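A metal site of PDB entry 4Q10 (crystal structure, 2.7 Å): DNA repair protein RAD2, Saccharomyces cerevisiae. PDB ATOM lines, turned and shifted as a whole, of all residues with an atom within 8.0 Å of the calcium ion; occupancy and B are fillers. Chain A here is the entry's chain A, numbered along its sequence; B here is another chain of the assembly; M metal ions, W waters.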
ATOM      1  N   GLY A   1     -23.933 -20.290  -3.456  1.00  0.00           N
ATOM      2  CA  GLY A   1     -24.429 -20.706  -4.759  1.00  0.00           C
ATOM      3  C   GLY A   1     -25.880 -20.329  -4.982  1.00  0.00           C
ATOM      4  O   GLY A   1     -26.650 -20.141  -4.026  1.00  0.00           O
ATOM      5  N   VAL A   2     -26.251 -20.174  -6.256  1.00  0.00           N
ATOM      6  CA  VAL A   2     -27.660 -20.040  -6.648  1.00  0.00           C
ATOM      7  C   VAL A   2     -28.103 -21.330  -7.323  1.00  0.00           C
ATOM      8  O   VAL A   2     -27.525 -21.743  -8.338  1.00  0.00           O
ATOM      9  CB  VAL A   2     -27.898 -18.841  -7.600  1.00  0.00           C
ATOM     10  CG1 VAL A   2     -29.259 -18.961  -8.287  1.00  0.00           C
ATOM     11  CG2 VAL A   2     -27.792 -17.532  -6.850  1.00  0.00           C
ATOM     12  N   ASP A  29     -10.947 -17.491  -5.803  1.00  0.00           N
ATOM     13  CA  ASP A  29     -11.884 -17.631  -4.708  1.00  0.00           C
ATOM     14  C   ASP A  29     -11.545 -18.922  -3.971  1.00  0.00           C
ATOM     15  O   ASP A  29     -11.803 -20.013  -4.465  1.00  0.00           O
ATOM     16  CB  ASP A  29     -13.323 -17.653  -5.238  1.00  0.00           C
ATOM     17  CG  ASP A  29     -14.359 -18.100  -4.183  1.00  0.00           C
ATOM     18  OD1 ASP A  29     -14.294 -17.635  -3.026  1.00  0.00           O
ATOM     19  OD2 ASP A  29     -15.229 -18.921  -4.545  1.00  0.00           O
ATOM     20  N   SER A  31     -12.425 -19.221  -0.668  1.00  0.00           N
ATOM     21  CA  SER A  31     -13.232 -19.057   0.538  1.00  0.00           C
ATOM     22  C   SER A  31     -13.565 -20.392   1.211  1.00  0.00           C
ATOM     23  O   SER A  31     -13.685 -20.446   2.436  1.00  0.00           O
ATOM     24  CB  SER A  31     -14.499 -18.242   0.231  1.00  0.00           C
ATOM     25  OG  SER A  31     -15.511 -19.017  -0.401  1.00  0.00           O
ATOM     26  N   ILE A  32     -13.692 -21.457   0.422  1.00  0.00           N
ATOM     27  CA  ILE A  32     -14.119 -22.758   0.945  1.00  0.00           C
ATOM     28  C   ILE A  32     -13.079 -23.858   0.765  1.00  0.00           C
ATOM     29  O   ILE A  32     -13.321 -25.003   1.168  1.00  0.00           O
ATOM     30  CB  ILE A  32     -15.419 -23.245   0.255  1.00  0.00           C
ATOM     31  CG1 ILE A  32     -15.242 -23.212  -1.267  1.00  0.00           C
ATOM     32  CG2 ILE A  32     -16.611 -22.414   0.719  1.00  0.00           C
ATOM     33  CD1 ILE A  32     -16.235 -24.033  -2.052  1.00  0.00           C
ATOM     34  N   ASP A  76     -12.799 -15.654   2.916  1.00  0.00           N
ATOM     35  CA  ASP A  76     -14.038 -15.124   3.515  1.00  0.00           C
ATOM     36  C   ASP A  76     -13.762 -14.277   4.749  1.00  0.00           C
ATOM     37  O   ASP A  76     -12.833 -14.553   5.512  1.00  0.00           O
ATOM     38  CB  ASP A  76     -15.001 -16.262   3.886  1.00  0.00           C
ATOM     39  CG  ASP A  76     -15.913 -16.647   2.743  1.00  0.00           C
ATOM     40  OD1 ASP A  76     -16.176 -15.787   1.886  1.00  0.00           O
ATOM     41  OD2 ASP A  76     -16.376 -17.812   2.711  1.00  0.00           O
ATOM     42  N   GLU A 171     -18.410 -11.736   1.914  1.00  0.00           N
ATOM     43  CA  GLU A 171     -18.271 -12.851   0.983  1.00  0.00           C
ATOM     44  C   GLU A 171     -17.159 -12.633  -0.035  1.00  0.00           C
ATOM     45  O   GLU A 171     -17.045 -11.548  -0.609  1.00  0.00           O
ATOM     46  CB  GLU A 171     -19.601 -13.133   0.272  1.00  0.00           C
ATOM     47  CG  GLU A 171     -20.480 -14.143   0.980  1.00  0.00           C
ATOM     48  CD  GLU A 171     -21.952 -13.926   0.697  1.00  0.00           C
ATOM     49  OE1 GLU A 171     -22.655 -14.901   0.323  1.00  0.00           O
ATOM     50  OE2 GLU A 171     -22.422 -12.777   0.858  1.00  0.00           O
ATOM     51  N   ALA A 172     -16.360 -13.666  -0.252  1.00  0.00           N
ATOM     52  CA  ALA A 172     -15.232 -13.622  -1.187  1.00  0.00           C
ATOM     53  C   ALA A 172     -15.676 -13.313  -2.612  1.00  0.00           C
ATOM     54  O   ALA A 172     -15.135 -12.416  -3.251  1.00  0.00           O
ATOM     55  CB  ALA A 172     -14.439 -14.919  -1.137  1.00  0.00           C
ATOM     56  N   GLU A 173     -16.656 -14.080  -3.111  1.00  0.00           N
ATOM     57  CA  GLU A 173     -17.161 -13.889  -4.463  1.00  0.00           C
ATOM     58  C   GLU A 173     -17.551 -12.433  -4.729  1.00  0.00           C
ATOM     59  O   GLU A 173     -17.333 -11.911  -5.818  1.00  0.00           O
ATOM     60  CB  GLU A 173     -18.372 -14.792  -4.742  1.00  0.00           C
ATOM     61  CG  GLU A 173     -18.460 -16.014  -3.854  1.00  0.00           C
ATOM     62  CD  GLU A 173     -19.262 -15.745  -2.599  1.00  0.00           C
ATOM     63  OE1 GLU A 173     -18.648 -15.516  -1.533  1.00  0.00           O
ATOM     64  OE2 GLU A 173     -20.511 -15.789  -2.669  1.00  0.00           O
ATOM     65  N   ALA A 174     -18.133 -11.792  -3.723  1.00  0.00           N
ATOM     66  CA  ALA A 174     -18.471 -10.373  -3.810  1.00  0.00           C
ATOM     67  C   ALA A 174     -17.210  -9.564  -4.035  1.00  0.00           C
ATOM     68  O   ALA A 174     -17.167  -8.718  -4.917  1.00  0.00           O
ATOM     69  CB  ALA A 174     -19.171  -9.910  -2.555  1.00  0.00           C
ATOM     70  N   THR A 190     -13.541 -19.272  -9.871  1.00  0.00           N
ATOM     71  CA  THR A 190     -14.464 -19.721  -8.846  1.00  0.00           C
ATOM     72  C   THR A 190     -15.412 -20.770  -9.403  1.00  0.00           C
ATOM     73  O   THR A 190     -15.532 -20.924 -10.617  1.00  0.00           O
ATOM     74  CB  THR A 190     -15.281 -18.554  -8.270  1.00  0.00           C
ATOM     75  OG1 THR A 190     -16.063 -19.018  -7.162  1.00  0.00           O
ATOM     76  CG2 THR A 190     -16.178 -17.956  -9.340  1.00  0.00           C
ATOM     77  N   ASP A 191     -16.067 -21.502  -8.505  1.00  0.00           N
ATOM     78  CA  ASP A 191     -17.078 -22.471  -8.890  1.00  0.00           C
ATOM     79  C   ASP A 191     -18.419 -22.061  -8.281  1.00  0.00           C
ATOM     80  O   ASP A 191     -19.409 -22.782  -8.399  1.00  0.00           O
ATOM     81  CB  ASP A 191     -16.664 -23.875  -8.429  1.00  0.00           C
ATOM     82  CG  ASP A 191     -15.815 -24.601  -9.462  1.00  0.00           C
ATOM     83  OD1 ASP A 191     -15.293 -23.939 -10.381  1.00  0.00           O
ATOM     84  OD2 ASP A 191     -15.670 -25.845  -9.349  1.00  0.00           O
ATOM     85  N   ASP A 192     -18.432 -20.897  -7.639  1.00  0.00           N
ATOM     86  CA  ASP A 192     -19.612 -20.377  -6.969  1.00  0.00           C
ATOM     87  C   ASP A 192     -20.375 -19.454  -7.922  1.00  0.00           C
ATOM     88  O   ASP A 192     -19.797 -18.492  -8.445  1.00  0.00           O
ATOM     89  CB  ASP A 192     -19.189 -19.602  -5.712  1.00  0.00           C
ATOM     90  CG  ASP A 192     -20.340 -19.332  -4.770  1.00  0.00           C
ATOM     91  OD1 ASP A 192     -20.613 -20.187  -3.905  1.00  0.00           O
ATOM     92  OD2 ASP A 192     -20.967 -18.273  -4.891  1.00  0.00           O
ATOM     93  N   SER A 193     -21.646 -19.746  -8.152  1.00  0.00           N
ATOM     94  CA  SER A 193     -22.401 -19.036  -9.189  1.00  0.00           C
ATOM     95  C   SER A 193     -22.887 -17.664  -8.753  1.00  0.00           C
ATOM     96  O   SER A 193     -23.264 -16.847  -9.591  1.00  0.00           O
ATOM     97  CB  SER A 193     -23.559 -19.893  -9.749  1.00  0.00           C
ATOM     98  OG  SER A 193     -24.615 -20.059  -8.821  1.00  0.00           O
ATOM     99  N   ASP A 194     -22.850 -17.388  -7.454  1.00  0.00           N
ATOM    100  CA  ASP A 194     -23.286 -16.102  -6.921  1.00  0.00           C
ATOM    101  C   ASP A 194     -22.472 -14.945  -7.454  1.00  0.00           C
ATOM    102  O   ASP A 194     -22.909 -13.790  -7.400  1.00  0.00           O
ATOM    103  CB  ASP A 194     -23.200 -16.076  -5.386  1.00  0.00           C
ATOM    104  CG  ASP A 194     -24.034 -17.147  -4.745  1.00  0.00           C
ATOM    105  OD1 ASP A 194     -24.873 -17.732  -5.470  1.00  0.00           O
ATOM    106  OD2 ASP A 194     -23.868 -17.415  -3.530  1.00  0.00           O
ATOM    107  N   VAL A 195     -21.285 -15.272  -7.960  1.00  0.00           N
ATOM    108  CA  VAL A 195     -20.367 -14.273  -8.484  1.00  0.00           C
ATOM    109  C   VAL A 195     -21.053 -13.455  -9.601  1.00  0.00           C
ATOM    110  O   VAL A 195     -20.874 -12.233  -9.675  1.00  0.00           O
ATOM    111  CB  VAL A 195     -19.002 -14.910  -8.907  1.00  0.00           C
ATOM    112  CG1 VAL A 195     -19.085 -15.612 -10.281  1.00  0.00           C
ATOM    113  CG2 VAL A 195     -17.904 -13.887  -8.882  1.00  0.00           C
ATOM    114  N   PHE A 198     -23.431 -10.795  -8.098  1.00  0.00           N
ATOM    115  CA  PHE A 198     -22.711  -9.670  -7.515  1.00  0.00           C
ATOM    116  C   PHE A 198     -22.117  -8.731  -8.582  1.00  0.00           C
ATOM    117  O   PHE A 198     -21.447  -7.764  -8.235  1.00  0.00           O
ATOM    118  CB  PHE A 198     -21.599 -10.156  -6.569  1.00  0.00           C
ATOM    119  CG  PHE A 198     -22.107 -10.719  -5.260  1.00  0.00           C
ATOM    120  CD1 PHE A 198     -22.771  -9.918  -4.349  1.00  0.00           C
ATOM    121  CD2 PHE A 198     -21.904 -12.057  -4.936  1.00  0.00           C
ATOM    122  CE1 PHE A 198     -23.233 -10.421  -3.151  1.00  0.00           C
ATOM    123  CE2 PHE A 198     -22.350 -12.580  -3.751  1.00  0.00           C
ATOM    124  CZ  PHE A 198     -23.022 -11.770  -2.847  1.00  0.00           C
ATOM    125  N   ASP A 243     -28.221 -18.552  -1.249  1.00  0.00           N
ATOM    126  CA  ASP A 243     -27.780 -18.228   0.111  1.00  0.00           C
ATOM    127  C   ASP A 243     -28.594 -17.088   0.731  1.00  0.00           C
ATOM    128  O   ASP A 243     -28.647 -16.962   1.950  1.00  0.00           O
ATOM    129  CB  ASP A 243     -26.287 -17.877   0.134  1.00  0.00           C
ATOM    130  CG  ASP A 243     -25.380 -19.094  -0.015  1.00  0.00           C
ATOM    131  OD1 ASP A 243     -25.860 -20.166  -0.436  1.00  0.00           O
ATOM    132  OD2 ASP A 243     -24.180 -18.963   0.276  1.00  0.00           O
ATOM    133  N   TYR A 244     -29.218 -16.265  -0.103  1.00  0.00           N
ATOM    134  CA  TYR A 244     -29.939 -15.087   0.371  1.00  0.00           C
ATOM    135  C   TYR A 244     -31.462 -15.270   0.429  1.00  0.00           C
ATOM    136  O   TYR A 244     -32.163 -14.452   1.042  1.00  0.00           O
ATOM    137  CB  TYR A 244     -29.604 -13.868  -0.492  1.00  0.00           C
ATOM    138  CG  TYR A 244     -28.188 -13.336  -0.360  1.00  0.00           C
ATOM    139  CD1 TYR A 244     -27.271 -13.940   0.483  1.00  0.00           C
ATOM    140  CD2 TYR A 244     -27.775 -12.214  -1.076  1.00  0.00           C
ATOM    141  CE1 TYR A 244     -25.979 -13.449   0.620  1.00  0.00           C
ATOM    142  CE2 TYR A 244     -26.493 -11.721  -0.953  1.00  0.00           C
ATOM    143  CZ  TYR A 244     -25.601 -12.340  -0.101  1.00  0.00           C
ATOM    144  OH  TYR A 244     -24.322 -11.860   0.036  1.00  0.00           O
ATOM    145  N   TYR A 317     -27.327  -7.987  -3.229  1.00  0.00           N
ATOM    146  CA  TYR A 317     -26.564  -8.401  -4.403  1.00  0.00           C
ATOM    147  C   TYR A 317     -25.968  -7.212  -5.155  1.00  0.00           C
ATOM    148  O   TYR A 317     -24.883  -7.334  -5.723  1.00  0.00           O
ATOM    149  CB  TYR A 317     -27.424  -9.232  -5.352  1.00  0.00           C
ATOM    150  CG  TYR A 317     -27.552 -10.695  -5.007  1.00  0.00           C
ATOM    151  CD1 TYR A 317     -26.434 -11.528  -4.973  1.00  0.00           C
ATOM    152  CD2 TYR A 317     -28.792 -11.259  -4.757  1.00  0.00           C
ATOM    153  CE1 TYR A 317     -26.552 -12.874  -4.671  1.00  0.00           C
ATOM    154  CE2 TYR A 317     -28.929 -12.600  -4.455  1.00  0.00           C
ATOM    155  CZ  TYR A 317     -27.804 -13.404  -4.409  1.00  0.00           C
ATOM    156  OH  TYR A 317     -27.930 -14.741  -4.115  1.00  0.00           O
ATOM    157  P    DC B   5     -22.269 -25.816   3.782  1.00  0.00           P
ATOM    158  OP1  DC B   5     -22.671 -25.262   2.466  1.00  0.00           O
ATOM    159  OP2  DC B   5     -23.188 -26.736   4.491  1.00  0.00           O
ATOM    160  O5'  DC B   5     -20.845 -26.543   3.640  1.00  0.00           O
ATOM    161  C5'  DC B   5     -19.689 -25.740   3.467  1.00  0.00           C
ATOM    162  C4'  DC B   5     -19.025 -26.024   2.129  1.00  0.00           C
ATOM    163  O4'  DC B   5     -18.384 -27.309   2.209  1.00  0.00           O
ATOM    164  C3'  DC B   5     -19.996 -26.074   0.950  1.00  0.00           C
ATOM    165  O3'  DC B   5     -19.762 -24.970   0.075  1.00  0.00           O
ATOM    166  C2'  DC B   5     -19.717 -27.412   0.260  1.00  0.00           C
ATOM    167  C1'  DC B   5     -18.532 -28.019   1.000  1.00  0.00           C
ATOM    168  N1   DC B   5     -18.686 -29.462   1.344  1.00  0.00           N
ATOM    169  C2   DC B   5     -18.253 -30.438   0.434  1.00  0.00           C
ATOM    170  O2   DC B   5     -17.771 -30.100  -0.646  1.00  0.00           O
ATOM    171  N3   DC B   5     -18.392 -31.746   0.776  1.00  0.00           N
ATOM    172  C4   DC B   5     -18.924 -32.078   1.956  1.00  0.00           C
ATOM    173  N4   DC B   5     -19.041 -33.380   2.255  1.00  0.00           N
ATOM    174  C5   DC B   5     -19.354 -31.086   2.893  1.00  0.00           C
ATOM    175  C6   DC B   5     -19.219 -29.800   2.546  1.00  0.00           C
ATOM    176  P    DT B   6     -20.949 -24.413  -0.867  1.00  0.00           P
ATOM    177  OP1  DT B   6     -20.362 -23.377  -1.750  1.00  0.00           O
ATOM    178  OP2  DT B   6     -22.100 -24.061  -0.002  1.00  0.00           O
ATOM    179  O5'  DT B   6     -21.365 -25.681  -1.743  1.00  0.00           O
ATOM    180  C5'  DT B   6     -21.527 -25.561  -3.145  1.00  0.00           C
ATOM    181  C4'  DT B   6     -20.824 -26.694  -3.864  1.00  0.00           C
ATOM    182  O4'  DT B   6     -20.432 -27.735  -2.932  1.00  0.00           O
ATOM    183  C3'  DT B   6     -21.675 -27.367  -4.931  1.00  0.00           C
ATOM    184  O3'  DT B   6     -20.904 -27.629  -6.094  1.00  0.00           O
ATOM    185  C2'  DT B   6     -22.119 -28.651  -4.238  1.00  0.00           C
ATOM    186  C1'  DT B   6     -20.867 -28.994  -3.447  1.00  0.00           C
ATOM    187  N1   DT B   6     -21.095 -29.996  -2.353  1.00  0.00           N
ATOM    188  C2   DT B   6     -20.632 -31.291  -2.517  1.00  0.00           C
ATOM    189  O2   DT B   6     -20.037 -31.677  -3.506  1.00  0.00           O
ATOM    190  N3   DT B   6     -20.905 -32.146  -1.468  1.00  0.00           N
ATOM    191  C4   DT B   6     -21.572 -31.837  -0.295  1.00  0.00           C
ATOM    192  O4   DT B   6     -21.765 -32.665   0.595  1.00  0.00           O
ATOM    193  C5   DT B   6     -22.027 -30.468  -0.185  1.00  0.00           C
ATOM    194  C7   DT B   6     -22.765 -30.034   1.051  1.00  0.00           C
ATOM    195  C6   DT B   6     -21.780 -29.633  -1.205  1.00  0.00           C
HETATM  196 CA    CA M   1     -21.546 -18.216  -2.561  1.00  0.00          CA
HETATM  197  O   HOH W   1     -21.397 -17.492  -0.175  1.00  0.00           O
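Water W1 lies within hydrogen-bond range of OE1 of Glu 171 (2.9 Å) and OD2 of Asp 243 (3.2 Å).
OD1 of Asp 192 sits close to N of Gly 1 (3.4 Å).
N of Asp 192 lies within hydrogen-bond range of OG1 of Thr 190, 3.1 Å away.
OD1 of Asp 194 sits close to N of Gly 1 (3.4 Å).
OD1 of Asp 194 lies within hydrogen-bond range of N of Val 2 (2.9 Å).
Merely in contact with the calcium ion: Gly 1 and Asp 243.
The nearest printed residue that does not touch the calcium ion is Glu 171 (4.5 Å).
The calcium ion is bound by OD2 of Asp 192 (2.4 Å), water W1 (2.5 Å), OD1 of Asp 192 (2.6 Å), OD2 of Asp 194 (2.6 Å) and OE2 of Glu 173 (2.6 Å).
The calcium ion has five donor atoms within binding distance.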
